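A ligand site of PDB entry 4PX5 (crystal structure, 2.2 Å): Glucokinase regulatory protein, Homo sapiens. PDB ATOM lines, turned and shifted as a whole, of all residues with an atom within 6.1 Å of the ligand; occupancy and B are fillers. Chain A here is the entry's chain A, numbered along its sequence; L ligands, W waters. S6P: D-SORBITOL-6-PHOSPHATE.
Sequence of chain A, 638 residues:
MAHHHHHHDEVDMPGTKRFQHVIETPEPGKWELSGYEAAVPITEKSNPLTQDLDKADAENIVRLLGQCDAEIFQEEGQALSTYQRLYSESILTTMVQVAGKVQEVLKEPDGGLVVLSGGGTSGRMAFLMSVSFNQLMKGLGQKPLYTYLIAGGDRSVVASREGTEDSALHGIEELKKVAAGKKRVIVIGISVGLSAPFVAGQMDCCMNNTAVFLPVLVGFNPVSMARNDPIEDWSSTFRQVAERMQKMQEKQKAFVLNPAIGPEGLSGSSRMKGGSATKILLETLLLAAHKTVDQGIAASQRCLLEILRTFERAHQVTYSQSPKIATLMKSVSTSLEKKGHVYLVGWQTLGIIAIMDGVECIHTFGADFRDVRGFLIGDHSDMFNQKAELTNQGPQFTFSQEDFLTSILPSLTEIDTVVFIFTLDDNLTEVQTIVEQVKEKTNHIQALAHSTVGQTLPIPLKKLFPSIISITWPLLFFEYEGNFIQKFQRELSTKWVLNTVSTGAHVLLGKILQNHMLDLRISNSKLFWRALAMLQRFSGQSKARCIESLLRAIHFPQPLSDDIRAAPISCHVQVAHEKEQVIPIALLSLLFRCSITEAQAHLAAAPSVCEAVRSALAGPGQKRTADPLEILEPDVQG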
ATOM      1  N   GLY A 119      24.319  -9.980   3.782  1.00  0.00           N
ATOM      2  CA  GLY A 119      25.548  -9.676   4.506  1.00  0.00           C
ATOM      3  C   GLY A 119      25.531 -10.487   5.768  1.00  0.00           C
ATOM      4  O   GLY A 119      24.439 -10.852   6.235  1.00  0.00           O
ATOM      5  N   GLY A 120      26.713 -10.823   6.266  1.00  0.00           N
ATOM      6  CA  GLY A 120      26.886 -11.489   7.540  1.00  0.00           C
ATOM      7  C   GLY A 120      26.071 -12.783   7.562  1.00  0.00           C
ATOM      8  O   GLY A 120      25.988 -13.451   6.536  1.00  0.00           O
ATOM      9  N   THR A 121      25.429 -13.099   8.694  1.00  0.00           N
ATOM     10  CA  THR A 121      24.670 -14.312   8.826  1.00  0.00           C
ATOM     11  C   THR A 121      23.620 -14.441   7.796  1.00  0.00           C
ATOM     12  O   THR A 121      23.317 -15.549   7.434  1.00  0.00           O
ATOM     13  CB  THR A 121      24.050 -14.465  10.180  1.00  0.00           C
ATOM     14  OG1 THR A 121      25.056 -14.244  11.122  1.00  0.00           O
ATOM     15  CG2 THR A 121      23.464 -15.879  10.425  1.00  0.00           C
ATOM     16  N   SER A 122      23.085 -13.343   7.241  1.00  0.00           N
ATOM     17  CA  SER A 122      22.177 -13.531   6.144  1.00  0.00           C
ATOM     18  C   SER A 122      22.815 -14.128   4.930  1.00  0.00           C
ATOM     19  O   SER A 122      22.182 -14.915   4.180  1.00  0.00           O
ATOM     20  CB  SER A 122      21.448 -12.240   5.742  1.00  0.00           C
ATOM     21  OG  SER A 122      20.523 -11.861   6.765  1.00  0.00           O
ATOM     22  N   ARG A 124      25.554 -16.181   5.125  1.00  0.00           N
ATOM     23  CA  ARG A 124      25.834 -17.507   5.486  1.00  0.00           C
ATOM     24  C   ARG A 124      24.595 -18.413   5.280  1.00  0.00           C
ATOM     25  O   ARG A 124      24.696 -19.498   4.713  1.00  0.00           O
ATOM     26  CB  ARG A 124      26.254 -17.524   6.933  1.00  0.00           C
ATOM     27  CG  ARG A 124      27.582 -16.857   7.196  1.00  0.00           C
ATOM     28  CD  ARG A 124      27.995 -17.078   8.629  1.00  0.00           C
ATOM     29  NE  ARG A 124      28.281 -15.827   9.338  1.00  0.00           N
ATOM     30  CZ  ARG A 124      29.444 -15.179   9.247  1.00  0.00           C
ATOM     31  NH1 ARG A 124      30.401 -15.655   8.470  1.00  0.00           N
ATOM     32  NH2 ARG A 124      29.628 -14.047   9.890  1.00  0.00           N
ATOM     33  N   GLU A 162      32.406  -7.794   9.363  1.00  0.00           N
ATOM     34  CA  GLU A 162      31.204  -6.947   9.550  1.00  0.00           C
ATOM     35  C   GLU A 162      31.188  -5.647   8.722  1.00  0.00           C
ATOM     36  O   GLU A 162      30.107  -5.139   8.424  1.00  0.00           O
ATOM     37  CB  GLU A 162      31.030  -6.608  11.032  1.00  0.00           C
ATOM     38  CG  GLU A 162      30.589  -7.774  11.875  1.00  0.00           C
ATOM     39  CD  GLU A 162      29.147  -8.169  11.556  1.00  0.00           C
ATOM     40  OE1 GLU A 162      28.232  -7.835  12.382  1.00  0.00           O
ATOM     41  OE2 GLU A 162      28.926  -8.788  10.471  1.00  0.00           O
ATOM     42  N   GLU A 165      29.158  -5.042   4.462  1.00  0.00           N
ATOM     43  CA  GLU A 165      27.737  -4.810   4.100  1.00  0.00           C
ATOM     44  C   GLU A 165      27.276  -3.361   3.674  1.00  0.00           C
ATOM     45  O   GLU A 165      26.147  -3.165   3.189  1.00  0.00           O
ATOM     46  CB  GLU A 165      26.830  -5.362   5.210  1.00  0.00           C
ATOM     47  CG  GLU A 165      26.823  -4.605   6.538  1.00  0.00           C
ATOM     48  CD  GLU A 165      25.658  -4.991   7.465  1.00  0.00           C
ATOM     49  OE1 GLU A 165      25.741  -6.059   8.115  1.00  0.00           O
ATOM     50  OE2 GLU A 165      24.678  -4.201   7.607  1.00  0.00           O
ATOM     51  N   ILE A 190      18.199 -10.912   1.376  1.00  0.00           N
ATOM     52  CA  ILE A 190      17.949 -11.222   2.718  1.00  0.00           C
ATOM     53  C   ILE A 190      18.633 -10.201   3.646  1.00  0.00           C
ATOM     54  O   ILE A 190      19.849 -10.146   3.740  1.00  0.00           O
ATOM     55  CB  ILE A 190      18.505 -12.626   3.007  1.00  0.00           C
ATOM     56  CG1 ILE A 190      17.951 -13.637   1.992  1.00  0.00           C
ATOM     57  CG2 ILE A 190      18.225 -12.945   4.435  1.00  0.00           C
ATOM     58  CD1 ILE A 190      18.587 -15.013   2.068  1.00  0.00           C
ATOM     59  N   SER A 191      17.830  -9.417   4.339  1.00  0.00           N
ATOM     60  CA  SER A 191      18.281  -8.525   5.382  1.00  0.00           C
ATOM     61  C   SER A 191      17.280  -8.499   6.528  1.00  0.00           C
ATOM     62  O   SER A 191      16.194  -7.915   6.456  1.00  0.00           O
ATOM     63  CB  SER A 191      18.481  -7.078   4.819  1.00  0.00           C
ATOM     64  OG  SER A 191      19.175  -6.305   5.789  1.00  0.00           O
ATOM     65  N   VAL A 192      17.669  -9.109   7.599  1.00  0.00           N
ATOM     66  CA  VAL A 192      16.808  -9.262   8.734  1.00  0.00           C
ATOM     67  C   VAL A 192      16.211  -7.980   9.165  1.00  0.00           C
ATOM     68  O   VAL A 192      14.988  -7.887   9.369  1.00  0.00           O
ATOM     69  CB  VAL A 192      17.594  -9.893   9.865  1.00  0.00           C
ATOM     70  CG1 VAL A 192      16.754  -9.867  11.138  1.00  0.00           C
ATOM     71  CG2 VAL A 192      17.883 -11.343   9.471  1.00  0.00           C
ATOM     72  N   GLY A 193      17.050  -6.969   9.293  1.00  0.00           N
ATOM     73  CA  GLY A 193      16.652  -5.669   9.759  1.00  0.00           C
ATOM     74  C   GLY A 193      16.068  -4.788   8.705  1.00  0.00           C
ATOM     75  O   GLY A 193      15.679  -3.657   9.006  1.00  0.00           O
ATOM     76  N   LEU A 194      16.031  -5.281   7.476  1.00  0.00           N
ATOM     77  CA  LEU A 194      15.711  -4.463   6.302  1.00  0.00           C
ATOM     78  C   LEU A 194      16.659  -3.246   6.334  1.00  0.00           C
ATOM     79  O   LEU A 194      16.224  -2.049   6.324  1.00  0.00           O
ATOM     80  CB  LEU A 194      14.257  -4.048   6.260  1.00  0.00           C
ATOM     81  CG  LEU A 194      13.189  -5.140   6.063  1.00  0.00           C
ATOM     82  CD1 LEU A 194      11.871  -4.528   5.611  1.00  0.00           C
ATOM     83  CD2 LEU A 194      13.617  -6.141   5.037  1.00  0.00           C
ATOM     84  N   SER A 195      17.939  -3.585   6.366  1.00  0.00           N
ATOM     85  CA  SER A 195      18.955  -2.685   6.741  1.00  0.00           C
ATOM     86  C   SER A 195      20.179  -2.607   5.829  1.00  0.00           C
ATOM     87  O   SER A 195      20.696  -1.528   5.696  1.00  0.00           O
ATOM     88  CB  SER A 195      19.462  -3.115   8.129  1.00  0.00           C
ATOM     89  OG  SER A 195      20.778  -2.742   8.281  1.00  0.00           O
ATOM     90  N   ALA A 196      20.640  -3.727   5.254  1.00  0.00           N
ATOM     91  CA  ALA A 196      21.967  -3.800   4.619  1.00  0.00           C
ATOM     92  C   ALA A 196      22.066  -3.054   3.277  1.00  0.00           C
ATOM     93  O   ALA A 196      21.275  -3.295   2.383  1.00  0.00           O
ATOM     94  CB  ALA A 196      22.394  -5.247   4.453  1.00  0.00           C
ATOM     95  N   VAL A 199      22.188  -5.143   0.203  1.00  0.00           N
ATOM     96  CA  VAL A 199      21.002  -5.720  -0.413  1.00  0.00           C
ATOM     97  C   VAL A 199      20.165  -4.686  -1.069  1.00  0.00           C
ATOM     98  O   VAL A 199      19.530  -4.943  -2.077  1.00  0.00           O
ATOM     99  CB  VAL A 199      20.138  -6.477   0.633  1.00  0.00           C
ATOM    100  CG1 VAL A 199      18.735  -6.780   0.079  1.00  0.00           C
ATOM    101  CG2 VAL A 199      20.864  -7.749   1.046  1.00  0.00           C
ATOM    102  N   GLY A 268      19.357  -6.958  19.021  1.00  0.00           N
ATOM    103  CA  GLY A 268      20.025  -6.795  17.762  1.00  0.00           C
ATOM    104  C   GLY A 268      20.904  -7.933  17.283  1.00  0.00           C
ATOM    105  O   GLY A 268      21.589  -7.775  16.304  1.00  0.00           O
ATOM    106  N   SER A 269      20.862  -9.105  17.914  1.00  0.00           N
ATOM    107  CA  SER A 269      21.751 -10.195  17.524  1.00  0.00           C
ATOM    108  C   SER A 269      20.973 -11.009  16.512  1.00  0.00           C
ATOM    109  O   SER A 269      20.470 -12.062  16.845  1.00  0.00           O
ATOM    110  CB  SER A 269      22.168 -11.054  18.724  1.00  0.00           C
ATOM    111  OG  SER A 269      23.101 -12.035  18.305  1.00  0.00           O
ATOM    112  N   SER A 270      20.852 -10.481  15.309  1.00  0.00           N
ATOM    113  CA  SER A 270      20.013 -11.043  14.307  1.00  0.00           C
ATOM    114  C   SER A 270      20.518 -12.370  13.702  1.00  0.00           C
ATOM    115  O   SER A 270      19.811 -13.011  12.898  1.00  0.00           O
ATOM    116  CB  SER A 270      19.793  -9.966  13.228  1.00  0.00           C
ATOM    117  OG  SER A 270      20.991  -9.689  12.639  1.00  0.00           O
ATOM    118  N   ARG A 271      21.707 -12.803  14.108  1.00  0.00           N
ATOM    119  CA  ARG A 271      22.208 -14.127  13.764  1.00  0.00           C
ATOM    120  C   ARG A 271      21.337 -15.238  14.331  1.00  0.00           C
ATOM    121  O   ARG A 271      21.349 -16.342  13.812  1.00  0.00           O
ATOM    122  CB  ARG A 271      23.623 -14.332  14.240  1.00  0.00           C
ATOM    123  CG  ARG A 271      23.858 -14.585  15.722  1.00  0.00           C
ATOM    124  CD  ARG A 271      25.354 -14.468  16.083  1.00  0.00           C
ATOM    125  NE  ARG A 271      25.531 -14.918  17.481  1.00  0.00           N
ATOM    126  CZ  ARG A 271      25.897 -16.157  17.880  1.00  0.00           C
ATOM    127  NH1 ARG A 271      26.341 -17.081  17.021  1.00  0.00           N
ATOM    128  NH2 ARG A 271      25.885 -16.434  19.181  1.00  0.00           N
ATOM    129  N   MET A 272      20.607 -14.938  15.391  1.00  0.00           N
ATOM    130  CA  MET A 272      19.824 -15.924  16.127  1.00  0.00           C
ATOM    131  C   MET A 272      18.465 -16.180  15.489  1.00  0.00           C
ATOM    132  O   MET A 272      18.381 -16.837  14.480  1.00  0.00           O
ATOM    133  CB  MET A 272      19.717 -15.437  17.582  1.00  0.00           C
ATOM    134  CG  MET A 272      21.085 -15.359  18.205  1.00  0.00           C
ATOM    135  SD  MET A 272      21.094 -14.858  19.927  1.00  0.00           S
ATOM    136  CE  MET A 272      20.885 -16.505  20.629  1.00  0.00           C
ATOM    137  N   GLU A 360      31.139 -16.104  14.415  1.00  0.00           N
ATOM    138  CA  GLU A 360      30.217 -15.070  14.837  1.00  0.00           C
ATOM    139  C   GLU A 360      30.478 -14.596  16.259  1.00  0.00           C
ATOM    140  O   GLU A 360      30.127 -13.448  16.578  1.00  0.00           O
ATOM    141  CB  GLU A 360      28.736 -15.479  14.653  1.00  0.00           C
ATOM    142  CG  GLU A 360      28.372 -15.559  13.192  1.00  0.00           C
ATOM    143  CD  GLU A 360      27.058 -16.248  12.910  1.00  0.00           C
ATOM    144  OE1 GLU A 360      26.521 -16.882  13.830  1.00  0.00           O
ATOM    145  OE2 GLU A 360      26.602 -16.158  11.747  1.00  0.00           O
ATOM    146  N   HIS A 363      32.926 -11.007  16.478  1.00  0.00           N
ATOM    147  CA  HIS A 363      32.249  -9.700  16.490  1.00  0.00           C
ATOM    148  C   HIS A 363      31.120  -9.683  17.506  1.00  0.00           C
ATOM    149  O   HIS A 363      30.924  -8.708  18.147  1.00  0.00           O
ATOM    150  CB  HIS A 363      31.821  -9.257  15.102  1.00  0.00           C
ATOM    151  CG  HIS A 363      30.864 -10.181  14.403  1.00  0.00           C
ATOM    152  ND1 HIS A 363      31.242 -11.004  13.364  1.00  0.00           N
ATOM    153  CD2 HIS A 363      29.528 -10.389  14.561  1.00  0.00           C
ATOM    154  CE1 HIS A 363      30.191 -11.673  12.908  1.00  0.00           C
ATOM    155  NE2 HIS A 363      29.144 -11.331  13.629  1.00  0.00           N
ATOM    156  N   THR A 364      30.422 -10.780  17.762  1.00  0.00           N
ATOM    157  CA  THR A 364      29.305 -10.651  18.708  1.00  0.00           C
ATOM    158  C   THR A 364      29.785 -10.341  20.107  1.00  0.00           C
ATOM    159  O   THR A 364      29.197  -9.509  20.769  1.00  0.00           O
ATOM    160  CB  THR A 364      28.432 -11.896  18.728  1.00  0.00           C
ATOM    161  OG1 THR A 364      27.979 -12.185  17.391  1.00  0.00           O
ATOM    162  CG2 THR A 364      27.225 -11.704  19.588  1.00  0.00           C
ATOM    163  N   ASN A 524      30.416  -1.248  11.308  1.00  0.00           N
ATOM    164  CA  ASN A 524      29.621  -0.749  10.200  1.00  0.00           C
ATOM    165  C   ASN A 524      28.675   0.302  10.728  1.00  0.00           C
ATOM    166  O   ASN A 524      28.582   0.471  11.935  1.00  0.00           O
ATOM    167  CB  ASN A 524      28.914  -1.901   9.426  1.00  0.00           C
ATOM    168  CG  ASN A 524      28.012  -2.782  10.295  1.00  0.00           C
ATOM    169  OD1 ASN A 524      27.980  -4.022  10.182  1.00  0.00           O
ATOM    170  ND2 ASN A 524      27.288  -2.189  11.120  1.00  0.00           N
ATOM    171  N   LYS A 526      25.348   0.390  10.751  1.00  0.00           N
ATOM    172  CA  LYS A 526      24.330  -0.153  11.663  1.00  0.00           C
ATOM    173  C   LYS A 526      24.796  -0.202  13.124  1.00  0.00           C
ATOM    174  O   LYS A 526      24.092   0.193  14.066  1.00  0.00           O
ATOM    175  CB  LYS A 526      23.917  -1.581  11.245  1.00  0.00           C
ATOM    176  CG  LYS A 526      22.833  -2.151  12.131  1.00  0.00           C
ATOM    177  CD  LYS A 526      22.247  -3.437  11.565  1.00  0.00           C
ATOM    178  CE  LYS A 526      23.263  -4.588  11.529  1.00  0.00           C
ATOM    179  NZ  LYS A 526      22.533  -5.664  10.858  1.00  0.00           N
ATOM    180  N   ARG A 530      23.517   1.622  16.557  1.00  0.00           N
ATOM    181  CA  ARG A 530      23.095   0.816  17.720  1.00  0.00           C
ATOM    182  C   ARG A 530      23.911   1.317  18.927  1.00  0.00           C
ATOM    183  O   ARG A 530      23.367   1.470  19.996  1.00  0.00           O
ATOM    184  CB  ARG A 530      23.233  -0.713  17.479  1.00  0.00           C
ATOM    185  CG  ARG A 530      22.840  -1.638  18.675  1.00  0.00           C
ATOM    186  CD  ARG A 530      23.105  -3.129  18.316  1.00  0.00           C
ATOM    187  NE  ARG A 530      22.354  -3.467  17.120  1.00  0.00           N
ATOM    188  CZ  ARG A 530      22.629  -4.410  16.217  1.00  0.00           C
ATOM    189  NH1 ARG A 530      23.669  -5.156  16.329  1.00  0.00           N
ATOM    190  NH2 ARG A 530      21.847  -4.569  15.153  1.00  0.00           N
HETATM  191  C1  S6P L   1      23.979 -10.134  13.524  1.00  0.00           C
HETATM  192  C2  S6P L   1      25.143 -10.559  12.595  1.00  0.00           C
HETATM  193  C3  S6P L   1      25.420  -9.609  11.465  1.00  0.00           C
HETATM  194  C4  S6P L   1      24.215  -9.545  10.579  1.00  0.00           C
HETATM  195  C5  S6P L   1      24.549  -8.695   9.376  1.00  0.00           C
HETATM  196  C6  S6P L   1      23.361  -8.670   8.445  1.00  0.00           C
HETATM  197  O1  S6P L   1      24.032 -10.998  14.745  1.00  0.00           O
HETATM  198  O2  S6P L   1      26.328 -10.678  13.347  1.00  0.00           O
HETATM  199  O3  S6P L   1      26.519 -10.153  10.736  1.00  0.00           O
HETATM  200  O4  S6P L   1      23.857 -10.875  10.151  1.00  0.00           O
HETATM  201  O5  S6P L   1      24.734  -7.372   9.908  1.00  0.00           O
HETATM  202  O6  S6P L   1      22.147  -8.235   9.183  1.00  0.00           O
HETATM  203  P   S6P L   1      20.913  -7.988   8.306  1.00  0.00           P
HETATM  204  O1P S6P L   1      19.815  -7.331   9.094  1.00  0.00           O
HETATM  205  O2P S6P L   1      21.123  -7.241   7.049  1.00  0.00           O
HETATM  206  O3P S6P L   1      20.434  -9.521   8.019  1.00  0.00           O
HETATM  207  O   HOH W   1      19.788  -6.592  11.459  1.00  0.00           O
HETATM  208  O   HOH W   2      21.885  -8.585   4.752  1.00  0.00           O
HETATM  209  O   HOH W   3      26.540  -6.141  11.715  1.00  0.00           O
HETATM  210  O   HOH W   4      22.219  -7.170  13.202  1.00  0.00           O
HETATM  211  O   HOH W   5      21.254 -10.931  10.028  1.00  0.00           O
HETATM  212  O   HOH W   6      27.790  -7.984   8.351  1.00  0.00           O
HETATM  213  O   HOH W   7      22.303  -4.964   8.133  1.00  0.00           O
HETATM  214  O   HOH W   8      27.427 -12.874  11.256  1.00  0.00           O
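The side-chain amide oxygen of Asn 524 sits close to the backbone carbonyl oxygen of Glu 162 (3.0 Å). The side-chain hydroxyl (OG) of Ser 191 sits at hydrogen-bond distance from the backbone NH (N) of Ser 195 (3.0 Å). The side-chain hydroxyl (OG1) of Thr 121 lies within hydrogen-bond range of the side-chain carboxylate (OE2) of Glu 360, 2.5 Å away. The backbone NH (N) of Lys 526 sits close to the side-chain amide nitrogen (ND2) of Asn 524 (3.2 Å). OG of Ser 191 is in hydrogen-bond range of N of Ala 196, 3.0 Å away. The guanidinium group (NH1) of Arg 271 lies within salt-bridge range of the side-chain carboxylate (OE1) of Glu 360 (3.2 Å).
Merely in contact with the ligand: Gly 119 (3.3 Å), Gly 120 (3.5 Å), Ala 196 (3.5 Å) and Ser 269 (3.5 Å). Hydrophobic or aromatic side chains that line the ligand: Val 192, Ala 196 and His 363. 15 residues have an atom within 4 Å of the ligand: Gly 119, Gly 120, Thr 121, Ser 122, Glu 162, Glu 165, Ser 191, Val 192, Gly 193, Ala 196, Ser 269, Ser 270, Arg 271, His 363 and Lys 526.
The side-chain carboxylate (OE2) of Glu 162 is in hydrogen-bond range of an oxygen (O3) of the ligand, at 2.8 Å. O3P of the ligand lies within hydrogen-bond range of N of Val 192. An oxygen (O1) of the ligand is in hydrogen-bond range of the backbone NH of Arg 271, 3.0 Å away. The backbone NH of Ser 270 sits at hydrogen-bond distance from an oxygen (O1) of the ligand. An oxygen (O3P) of the ligand lies within hydrogen-bond range of the side-chain hydroxyl (OG) of Ser 122, 2.7 Å away. The backbone NH of Thr 121 lies within hydrogen-bond range of an oxygen (O4) of the ligand (3.1 Å). OG of Ser 191 is in hydrogen-bond range of O2P of the ligand (2.5 Å). A ring nitrogen (NE2) of His 363 lies within hydrogen-bond range of an oxygen (O2) of the ligand (2.9 Å). The backbone NH (N) of Gly 193 lies within hydrogen-bond range of an oxygen (O1P) of the ligand (2.8 Å). The side-chain carboxylate (OE1) of Glu 165 is in hydrogen-bond range of an oxygen (O5) of the ligand (2.4 Å). NZ of Lys 526 lies within salt-bridge range of O1P of the ligand, 3.6 Å away.
Water W1 bridges an oxygen (O1P) of the ligand (2.5 Å) and the side-chain amino group (NZ) of Lys 526 (3.0 Å). Water W2 lies within hydrogen-bond range of the backbone carbonyl oxygen (O) of Ile 190 (2.8 Å), an oxygen (O2P) of the ligand (2.8 Å) and the backbone NH (N) of Gly 119 (3.0 Å). Water W7 lies within hydrogen-bond range of OE2 of Glu 165 (2.5 Å), OG of Ser 195 (2.7 Å), O2P of the ligand (2.8 Å) and NZ of Lys 526 (2.8 Å). Water W3 lies within hydrogen-bond range of OE1 of Glu 162 (2.5 Å), O5 of the ligand (2.8 Å) and OD1 of Asn 524 (3.0 Å). Water W8 lies within hydrogen-bond range of OG1 of Thr 121 (2.7 Å), NH2 of Arg 124 (2.8 Å), O3 of the ligand (2.9 Å), NE2 of His 363 (3.3 Å) and OE2 of Glu 360 (3.4 Å). Water W6 lies within hydrogen-bond range of the side-chain carboxylate of Glu 162 (2.5 Å), the side-chain carboxylate of Glu 165 (2.8 Å) and an oxygen (O3) of the ligand (3.5 Å).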
